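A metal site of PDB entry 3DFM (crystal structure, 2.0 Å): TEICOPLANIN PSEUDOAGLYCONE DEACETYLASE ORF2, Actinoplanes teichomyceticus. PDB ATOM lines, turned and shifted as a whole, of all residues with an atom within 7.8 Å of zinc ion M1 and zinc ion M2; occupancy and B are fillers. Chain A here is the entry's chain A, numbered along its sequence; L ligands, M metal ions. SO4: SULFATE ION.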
ATOM      1  N   SER A  14     -15.952 -28.854 -26.708  1.00  0.00           N
ATOM      2  CA  SER A  14     -16.944 -28.276 -25.806  1.00  0.00           C
ATOM      3  C   SER A  14     -17.017 -26.757 -26.015  1.00  0.00           C
ATOM      4  O   SER A  14     -15.987 -26.084 -26.080  1.00  0.00           O
ATOM      5  CB  SER A  14     -16.533 -28.584 -24.362  1.00  0.00           C
ATOM      6  OG  SER A  14     -17.526 -28.211 -23.435  1.00  0.00           O
ATOM      7  N   PRO A  15     -18.235 -26.198 -26.136  1.00  0.00           N
ATOM      8  CA  PRO A  15     -18.295 -24.735 -26.248  1.00  0.00           C
ATOM      9  C   PRO A  15     -17.779 -24.072 -24.970  1.00  0.00           C
ATOM     10  O   PRO A  15     -16.923 -23.194 -25.027  1.00  0.00           O
ATOM     11  CB  PRO A  15     -19.776 -24.442 -26.461  1.00  0.00           C
ATOM     12  CG  PRO A  15     -20.394 -25.754 -26.834  1.00  0.00           C
ATOM     13  CD  PRO A  15     -19.575 -26.809 -26.165  1.00  0.00           C
ATOM     14  N   HIS A  16     -18.274 -24.526 -23.814  1.00  0.00           N
ATOM     15  CA  HIS A  16     -17.945 -23.884 -22.550  1.00  0.00           C
ATOM     16  C   HIS A  16     -17.322 -24.887 -21.604  1.00  0.00           C
ATOM     17  O   HIS A  16     -17.448 -26.091 -21.800  1.00  0.00           O
ATOM     18  CB  HIS A  16     -19.212 -23.311 -21.860  1.00  0.00           C
ATOM     19  CG  HIS A  16     -19.962 -22.295 -22.677  1.00  0.00           C
ATOM     20  ND1 HIS A  16     -21.225 -22.533 -23.175  1.00  0.00           N
ATOM     21  CD2 HIS A  16     -19.626 -21.045 -23.062  1.00  0.00           C
ATOM     22  CE1 HIS A  16     -21.629 -21.458 -23.840  1.00  0.00           C
ATOM     23  NE2 HIS A  16     -20.682 -20.547 -23.779  1.00  0.00           N
ATOM     24  N   LEU A  17     -16.693 -24.382 -20.555  1.00  0.00           N
ATOM     25  CA  LEU A  17     -16.156 -25.198 -19.487  1.00  0.00           C
ATOM     26  C   LEU A  17     -17.305 -25.810 -18.674  1.00  0.00           C
ATOM     27  O   LEU A  17     -17.827 -25.174 -17.767  1.00  0.00           O
ATOM     28  CB  LEU A  17     -15.241 -24.336 -18.598  1.00  0.00           C
ATOM     29  CG  LEU A  17     -14.017 -23.721 -19.315  1.00  0.00           C
ATOM     30  CD1 LEU A  17     -13.447 -22.511 -18.598  1.00  0.00           C
ATOM     31  CD2 LEU A  17     -12.891 -24.777 -19.540  1.00  0.00           C
ATOM     32  N   ASP A  18     -17.709 -27.014 -19.058  1.00  0.00           N
ATOM     33  CA  ASP A  18     -18.741 -27.859 -18.409  1.00  0.00           C
ATOM     34  C   ASP A  18     -19.621 -28.639 -19.385  1.00  0.00           C
ATOM     35  O   ASP A  18     -20.179 -29.662 -19.014  1.00  0.00           O
ATOM     36  CB  ASP A  18     -19.583 -27.120 -17.326  1.00  0.00           C
ATOM     37  CG  ASP A  18     -20.526 -26.067 -17.902  1.00  0.00           C
ATOM     38  OD1 ASP A  18     -20.537 -25.817 -19.128  1.00  0.00           O
ATOM     39  OD2 ASP A  18     -21.277 -25.462 -17.088  1.00  0.00           O
ATOM     40  N   ASP A  19     -19.750 -28.164 -20.625  1.00  0.00           N
ATOM     41  CA  ASP A  19     -20.685 -28.784 -21.582  1.00  0.00           C
ATOM     42  C   ASP A  19     -20.387 -30.249 -21.941  1.00  0.00           C
ATOM     43  O   ASP A  19     -21.286 -31.072 -22.008  1.00  0.00           O
ATOM     44  CB  ASP A  19     -20.760 -27.970 -22.873  1.00  0.00           C
ATOM     45  CG  ASP A  19     -21.400 -26.626 -22.688  1.00  0.00           C
ATOM     46  OD1 ASP A  19     -22.458 -26.537 -22.025  1.00  0.00           O
ATOM     47  OD2 ASP A  19     -20.839 -25.648 -23.196  1.00  0.00           O
ATOM     48  N   ALA A  20     -19.111 -30.556 -22.206  1.00  0.00           N
ATOM     49  CA  ALA A  20     -18.693 -31.926 -22.535  1.00  0.00           C
ATOM     50  C   ALA A  20     -18.994 -32.866 -21.379  1.00  0.00           C
ATOM     51  O   ALA A  20     -19.468 -33.975 -21.589  1.00  0.00           O
ATOM     52  CB  ALA A  20     -17.192 -31.969 -22.868  1.00  0.00           C
ATOM     53  N   LEU A  22     -21.178 -32.430 -18.757  1.00  0.00           N
ATOM     54  CA  LEU A  22     -22.645 -32.509 -18.569  1.00  0.00           C
ATOM     55  C   LEU A  22     -23.353 -33.380 -19.611  1.00  0.00           C
ATOM     56  O   LEU A  22     -24.257 -34.162 -19.276  1.00  0.00           O
ATOM     57  CB  LEU A  22     -23.242 -31.095 -18.625  1.00  0.00           C
ATOM     58  CG  LEU A  22     -23.018 -30.198 -17.400  1.00  0.00           C
ATOM     59  CD1 LEU A  22     -23.204 -28.743 -17.794  1.00  0.00           C
ATOM     60  CD2 LEU A  22     -23.989 -30.585 -16.272  1.00  0.00           C
ATOM     61  N   PHE A  44     -14.517 -21.743 -25.862  1.00  0.00           N
ATOM     62  CA  PHE A  44     -14.658 -20.472 -25.168  1.00  0.00           C
ATOM     63  C   PHE A  44     -14.052 -20.465 -23.762  1.00  0.00           C
ATOM     64  O   PHE A  44     -14.732 -20.267 -22.765  1.00  0.00           O
ATOM     65  CB  PHE A  44     -16.127 -19.950 -25.221  1.00  0.00           C
ATOM     66  CG  PHE A  44     -16.570 -19.659 -26.607  1.00  0.00           C
ATOM     67  CD1 PHE A  44     -16.197 -18.489 -27.228  1.00  0.00           C
ATOM     68  CD2 PHE A  44     -17.268 -20.613 -27.328  1.00  0.00           C
ATOM     69  CE1 PHE A  44     -16.553 -18.236 -28.538  1.00  0.00           C
ATOM     70  CE2 PHE A  44     -17.645 -20.361 -28.657  1.00  0.00           C
ATOM     71  CZ  PHE A  44     -17.279 -19.180 -29.260  1.00  0.00           C
ATOM     72  N   ARG A  75     -12.720 -20.997 -13.445  1.00  0.00           N
ATOM     73  CA  ARG A  75     -13.484 -21.983 -14.218  1.00  0.00           C
ATOM     74  C   ARG A  75     -12.599 -22.986 -14.972  1.00  0.00           C
ATOM     75  O   ARG A  75     -12.965 -24.148 -15.137  1.00  0.00           O
ATOM     76  CB  ARG A  75     -14.468 -21.265 -15.134  1.00  0.00           C
ATOM     77  CG  ARG A  75     -15.536 -20.555 -14.295  1.00  0.00           C
ATOM     78  CD  ARG A  75     -16.809 -20.347 -15.014  1.00  0.00           C
ATOM     79  NE  ARG A  75     -17.336 -21.579 -15.588  1.00  0.00           N
ATOM     80  CZ  ARG A  75     -18.273 -21.599 -16.534  1.00  0.00           C
ATOM     81  NH1 ARG A  75     -18.778 -20.455 -16.977  1.00  0.00           N
ATOM     82  NH2 ARG A  75     -18.707 -22.745 -17.016  1.00  0.00           N
ATOM     83  N   LEU A  96     -12.813 -15.859 -26.435  1.00  0.00           N
ATOM     84  CA  LEU A  96     -13.440 -15.195 -25.299  1.00  0.00           C
ATOM     85  C   LEU A  96     -14.926 -15.514 -25.262  1.00  0.00           C
ATOM     86  O   LEU A  96     -15.633 -15.349 -26.265  1.00  0.00           O
ATOM     87  CB  LEU A  96     -13.214 -13.681 -25.341  1.00  0.00           C
ATOM     88  CG  LEU A  96     -11.801 -13.121 -25.188  1.00  0.00           C
ATOM     89  CD1 LEU A  96     -11.776 -11.609 -25.429  1.00  0.00           C
ATOM     90  CD2 LEU A  96     -11.224 -13.465 -23.830  1.00  0.00           C
ATOM     91  N   ASP A  97     -15.415 -15.970 -24.113  1.00  0.00           N
ATOM     92  CA  ASP A  97     -16.829 -16.243 -23.980  1.00  0.00           C
ATOM     93  C   ASP A  97     -17.662 -14.992 -24.269  1.00  0.00           C
ATOM     94  O   ASP A  97     -17.163 -13.881 -24.162  1.00  0.00           O
ATOM     95  CB  ASP A  97     -17.146 -16.780 -22.582  1.00  0.00           C
ATOM     96  CG  ASP A  97     -18.490 -17.455 -22.530  1.00  0.00           C
ATOM     97  OD1 ASP A  97     -19.027 -17.786 -23.608  1.00  0.00           O
ATOM     98  OD2 ASP A  97     -19.012 -17.642 -21.426  1.00  0.00           O
ATOM     99  N   SER A  98     -18.935 -15.191 -24.634  1.00  0.00           N
ATOM    100  CA  SER A  98     -19.847 -14.101 -25.024  1.00  0.00           C
ATOM    101  C   SER A  98     -19.808 -12.846 -24.117  1.00  0.00           C
ATOM    102  O   SER A  98     -19.855 -11.720 -24.630  1.00  0.00           O
ATOM    103  CB  SER A  98     -21.282 -14.638 -25.133  1.00  0.00           C
ATOM    104  OG  SER A  98     -21.777 -14.910 -23.843  1.00  0.00           O
ATOM    105  N   ILE A  99     -19.721 -13.032 -22.810  1.00  0.00           N
ATOM    106  CA  ILE A  99     -19.766 -11.898 -21.853  1.00  0.00           C
ATOM    107  C   ILE A  99     -18.482 -11.066 -21.820  1.00  0.00           C
ATOM    108  O   ILE A  99     -18.418 -10.027 -21.155  1.00  0.00           O
ATOM    109  CB  ILE A  99     -20.070 -12.335 -20.372  1.00  0.00           C
ATOM    110  CG1 ILE A  99     -19.256 -13.580 -19.977  1.00  0.00           C
ATOM    111  CG2 ILE A  99     -21.564 -12.585 -20.152  1.00  0.00           C
ATOM    112  CD1 ILE A  99     -19.151 -13.783 -18.468  1.00  0.00           C
ATOM    113  N   ARG A 101     -16.663 -10.559 -24.982  1.00  0.00           N
ATOM    114  CA  ARG A 101     -16.413 -10.082 -26.344  1.00  0.00           C
ATOM    115  C   ARG A 101     -16.982  -8.678 -26.566  1.00  0.00           C
ATOM    116  O   ARG A 101     -18.005  -8.295 -25.975  1.00  0.00           O
ATOM    117  CB  ARG A 101     -16.999 -11.052 -27.387  1.00  0.00           C
ATOM    118  CG  ARG A 101     -16.417 -12.452 -27.305  1.00  0.00           C
ATOM    119  CD  ARG A 101     -16.577 -13.253 -28.607  1.00  0.00           C
ATOM    120  NE  ARG A 101     -17.957 -13.611 -28.948  1.00  0.00           N
ATOM    121  CZ  ARG A 101     -18.647 -14.638 -28.462  1.00  0.00           C
ATOM    122  NH1 ARG A 101     -18.123 -15.437 -27.550  1.00  0.00           N
ATOM    123  NH2 ARG A 101     -19.880 -14.871 -28.879  1.00  0.00           N
ATOM    124  N   CYS A 155     -21.130 -30.461 -29.705  1.00  0.00           N
ATOM    125  CA  CYS A 155     -22.527 -30.223 -29.270  1.00  0.00           C
ATOM    126  C   CYS A 155     -23.497 -30.063 -30.446  1.00  0.00           C
ATOM    127  O   CYS A 155     -23.134 -29.487 -31.465  1.00  0.00           O
ATOM    128  CB  CYS A 155     -22.590 -28.945 -28.409  1.00  0.00           C
ATOM    129  SG  CYS A 155     -22.022 -27.460 -29.235  1.00  0.00           S
ATOM    130  N   HIS A 161     -27.991 -21.906 -28.050  1.00  0.00           N
ATOM    131  CA  HIS A 161     -27.007 -20.981 -27.515  1.00  0.00           C
ATOM    132  C   HIS A 161     -26.028 -20.573 -28.641  1.00  0.00           C
ATOM    133  O   HIS A 161     -25.537 -21.446 -29.349  1.00  0.00           O
ATOM    134  CB  HIS A 161     -26.241 -21.623 -26.363  1.00  0.00           C
ATOM    135  CG  HIS A 161     -25.548 -20.637 -25.503  1.00  0.00           C
ATOM    136  ND1 HIS A 161     -24.515 -19.854 -25.969  1.00  0.00           N
ATOM    137  CD2 HIS A 161     -25.738 -20.290 -24.214  1.00  0.00           C
ATOM    138  CE1 HIS A 161     -24.100 -19.054 -24.999  1.00  0.00           C
ATOM    139  NE2 HIS A 161     -24.817 -19.307 -23.919  1.00  0.00           N
ATOM    140  N   PRO A 162     -25.806 -19.252 -28.844  1.00  0.00           N
ATOM    141  CA  PRO A 162     -24.949 -18.809 -29.954  1.00  0.00           C
ATOM    142  C   PRO A 162     -23.528 -19.370 -29.909  1.00  0.00           C
ATOM    143  O   PRO A 162     -22.954 -19.690 -30.959  1.00  0.00           O
ATOM    144  CB  PRO A 162     -24.947 -17.277 -29.805  1.00  0.00           C
ATOM    145  CG  PRO A 162     -26.210 -16.977 -29.068  1.00  0.00           C
ATOM    146  CD  PRO A 162     -26.360 -18.114 -28.096  1.00  0.00           C
ATOM    147  N   ASP A 163     -22.961 -19.490 -28.714  1.00  0.00           N
ATOM    148  CA  ASP A 163     -21.611 -20.065 -28.579  1.00  0.00           C
ATOM    149  C   ASP A 163     -21.588 -21.565 -28.865  1.00  0.00           C
ATOM    150  O   ASP A 163     -20.578 -22.093 -29.306  1.00  0.00           O
ATOM    151  CB  ASP A 163     -21.020 -19.753 -27.210  1.00  0.00           C
ATOM    152  CG  ASP A 163     -20.764 -18.258 -27.010  1.00  0.00           C
ATOM    153  OD1 ASP A 163     -20.644 -17.534 -28.014  1.00  0.00           O
ATOM    154  OD2 ASP A 163     -20.716 -17.823 -25.842  1.00  0.00           O
ATOM    155  N   HIS A 164     -22.713 -22.239 -28.610  1.00  0.00           N
ATOM    156  CA  HIS A 164     -22.866 -23.656 -28.970  1.00  0.00           C
ATOM    157  C   HIS A 164     -22.980 -23.842 -30.484  1.00  0.00           C
ATOM    158  O   HIS A 164     -22.404 -24.774 -31.071  1.00  0.00           O
ATOM    159  CB  HIS A 164     -24.079 -24.256 -28.247  1.00  0.00           C
ATOM    160  CG  HIS A 164     -23.859 -24.491 -26.777  1.00  0.00           C
ATOM    161  ND1 HIS A 164     -24.420 -25.554 -26.094  1.00  0.00           N
ATOM    162  CD2 HIS A 164     -23.147 -23.808 -25.862  1.00  0.00           C
ATOM    163  CE1 HIS A 164     -24.055 -25.515 -24.836  1.00  0.00           C
ATOM    164  NE2 HIS A 164     -23.271 -24.460 -24.658  1.00  0.00           N
ATOM    165  N   THR A 167     -19.514 -23.182 -32.091  1.00  0.00           N
ATOM    166  CA  THR A 167     -18.604 -24.301 -31.833  1.00  0.00           C
ATOM    167  C   THR A 167     -18.930 -25.449 -32.770  1.00  0.00           C
ATOM    168  O   THR A 167     -18.043 -25.990 -33.432  1.00  0.00           O
ATOM    169  CB  THR A 167     -18.716 -24.788 -30.370  1.00  0.00           C
ATOM    170  OG1 THR A 167     -18.271 -23.757 -29.502  1.00  0.00           O
ATOM    171  CG2 THR A 167     -17.850 -26.023 -30.138  1.00  0.00           C
ATOM    172  N   ASP A 187     -27.239 -31.709 -26.054  1.00  0.00           N
ATOM    173  CA  ASP A 187     -26.843 -30.702 -25.058  1.00  0.00           C
ATOM    174  C   ASP A 187     -27.629 -30.844 -23.752  1.00  0.00           C
ATOM    175  O   ASP A 187     -28.861 -30.792 -23.769  1.00  0.00           O
ATOM    176  CB  ASP A 187     -27.038 -29.275 -25.578  1.00  0.00           C
ATOM    177  CG  ASP A 187     -26.378 -29.044 -26.940  1.00  0.00           C
ATOM    178  OD1 ASP A 187     -25.478 -28.185 -27.035  1.00  0.00           O
ATOM    179  OD2 ASP A 187     -26.758 -29.738 -27.904  1.00  0.00           O
ATOM    180  N   LEU A 188     -26.926 -31.019 -22.640  1.00  0.00           N
ATOM    181  CA  LEU A 188     -27.574 -31.086 -21.323  1.00  0.00           C
ATOM    182  C   LEU A 188     -27.058 -29.992 -20.391  1.00  0.00           C
ATOM    183  O   LEU A 188     -25.879 -29.629 -20.460  1.00  0.00           O
ATOM    184  CB  LEU A 188     -27.385 -32.455 -20.685  1.00  0.00           C
ATOM    185  CG  LEU A 188     -27.956 -33.679 -21.399  1.00  0.00           C
ATOM    186  CD1 LEU A 188     -27.525 -34.943 -20.646  1.00  0.00           C
ATOM    187  CD2 LEU A 188     -29.470 -33.607 -21.529  1.00  0.00           C
ATOM    188  N   TYR A 190     -29.825 -28.519 -21.294  1.00  0.00           N
ATOM    189  CA  TYR A 190     -30.687 -27.863 -22.288  1.00  0.00           C
ATOM    190  C   TYR A 190     -31.829 -28.731 -22.790  1.00  0.00           C
ATOM    191  O   TYR A 190     -32.982 -28.274 -22.838  1.00  0.00           O
ATOM    192  CB  TYR A 190     -29.867 -27.383 -23.497  1.00  0.00           C
ATOM    193  CG  TYR A 190     -28.912 -26.246 -23.210  1.00  0.00           C
ATOM    194  CD1 TYR A 190     -29.281 -24.918 -23.436  1.00  0.00           C
ATOM    195  CD2 TYR A 190     -27.623 -26.494 -22.715  1.00  0.00           C
ATOM    196  CE1 TYR A 190     -28.415 -23.872 -23.180  1.00  0.00           C
ATOM    197  CE2 TYR A 190     -26.740 -25.441 -22.446  1.00  0.00           C
ATOM    198  CZ  TYR A 190     -27.151 -24.141 -22.688  1.00  0.00           C
ATOM    199  OH  TYR A 190     -26.315 -23.083 -22.463  1.00  0.00           O
HETATM  200  S   SO4 L   1     -23.528 -23.880 -20.051  1.00  0.00           S
HETATM  201  O1  SO4 L   1     -24.026 -25.130 -19.540  1.00  0.00           O
HETATM  202  O2  SO4 L   1     -22.087 -23.762 -19.940  1.00  0.00           O
HETATM  203  O3  SO4 L   1     -24.069 -23.752 -21.391  1.00  0.00           O
HETATM  204  O4  SO4 L   1     -24.025 -22.706 -19.358  1.00  0.00           O
HETATM  205  S   SO4 L   2     -22.524 -17.807 -21.571  1.00  0.00           S
HETATM  206  O1  SO4 L   2     -22.132 -16.685 -20.747  1.00  0.00           O
HETATM  207  O2  SO4 L   2     -22.066 -17.553 -22.904  1.00  0.00           O
HETATM  208  O3  SO4 L   2     -21.982 -18.972 -20.894  1.00  0.00           O
HETATM  209  O4  SO4 L   2     -23.964 -17.896 -21.634  1.00  0.00           O
HETATM  210 ZN    ZN M   1     -22.346 -24.078 -22.915  1.00  0.00          ZN
HETATM  211 ZN    ZN M   2     -20.663 -18.554 -24.122  1.00  0.00          ZN
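The side-chain carboxylate (OD2) of Asp 163 sits close to the backbone NH (N) of Ser 98 (3.4 Å). The guanidinium group of Arg 101 is in salt-bridge range of the side-chain carboxylate of Asp 163 (2.9 Å). A ring nitrogen (ND1) of His 164 sits at hydrogen-bond distance from the side-chain carboxylate (OD1) of Asp 187. The backbone carbonyl oxygen (O) of His 16 is in hydrogen-bond range of the side-chain hydroxyl (OG) of Ser 14 (2.7 Å). The backbone carbonyl oxygen (O) of Asp 163 sits at hydrogen-bond distance from the side-chain hydroxyl (OG1) of Thr 167. The backbone NH of Asp 163 lies within hydrogen-bond range of a ring nitrogen (ND1) of His 161. The side-chain sulfur (SG) of Cys 155 is in hydrogen-bond range of the backbone carbonyl oxygen (O) of His 164, 3.3 Å away.
Within 4 Å of zinc ion M1: His 16, Asp 19 and His 164. Along chain A the residues within 4 Å of zinc ion M1 span positions 16 to 164.
Residues that only touch zinc ion M2: Ser 98 (3.8 Å) and His 161 (3.6 Å). Within 4 Å of zinc ion M2: His 16, Asp 97, Ser 98, His 161 and Asp 163. Along chain A the residues within 4 Å of zinc ion M2 span positions 16 to 163.
Zinc ion M1 is bound by ND1 of His 16 (1.9 Å), NE2 of His 164 (2.0 Å), OD2 of Asp 19 (2.2 Å) and O3 of SO4 L1 (2.3 Å). Zinc ion M1 has four donor atoms within binding distance. Slightly farther from zinc ion M1 lies the side-chain carboxylate (OD1) of Asp 19 (2.6 Å).
OD2 of Asp 163 binds zinc ion M2, at 1.9 Å. The side-chain carboxylate (OD1) of Asp 97 is bound to zinc ion M2, 1.9 Å away. A ring nitrogen (NE2) of His 16 is bound to zinc ion M2 (2.0 Å). Zinc ion M2 is bound by O2 of SO4 L2, at 2.1 Å.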
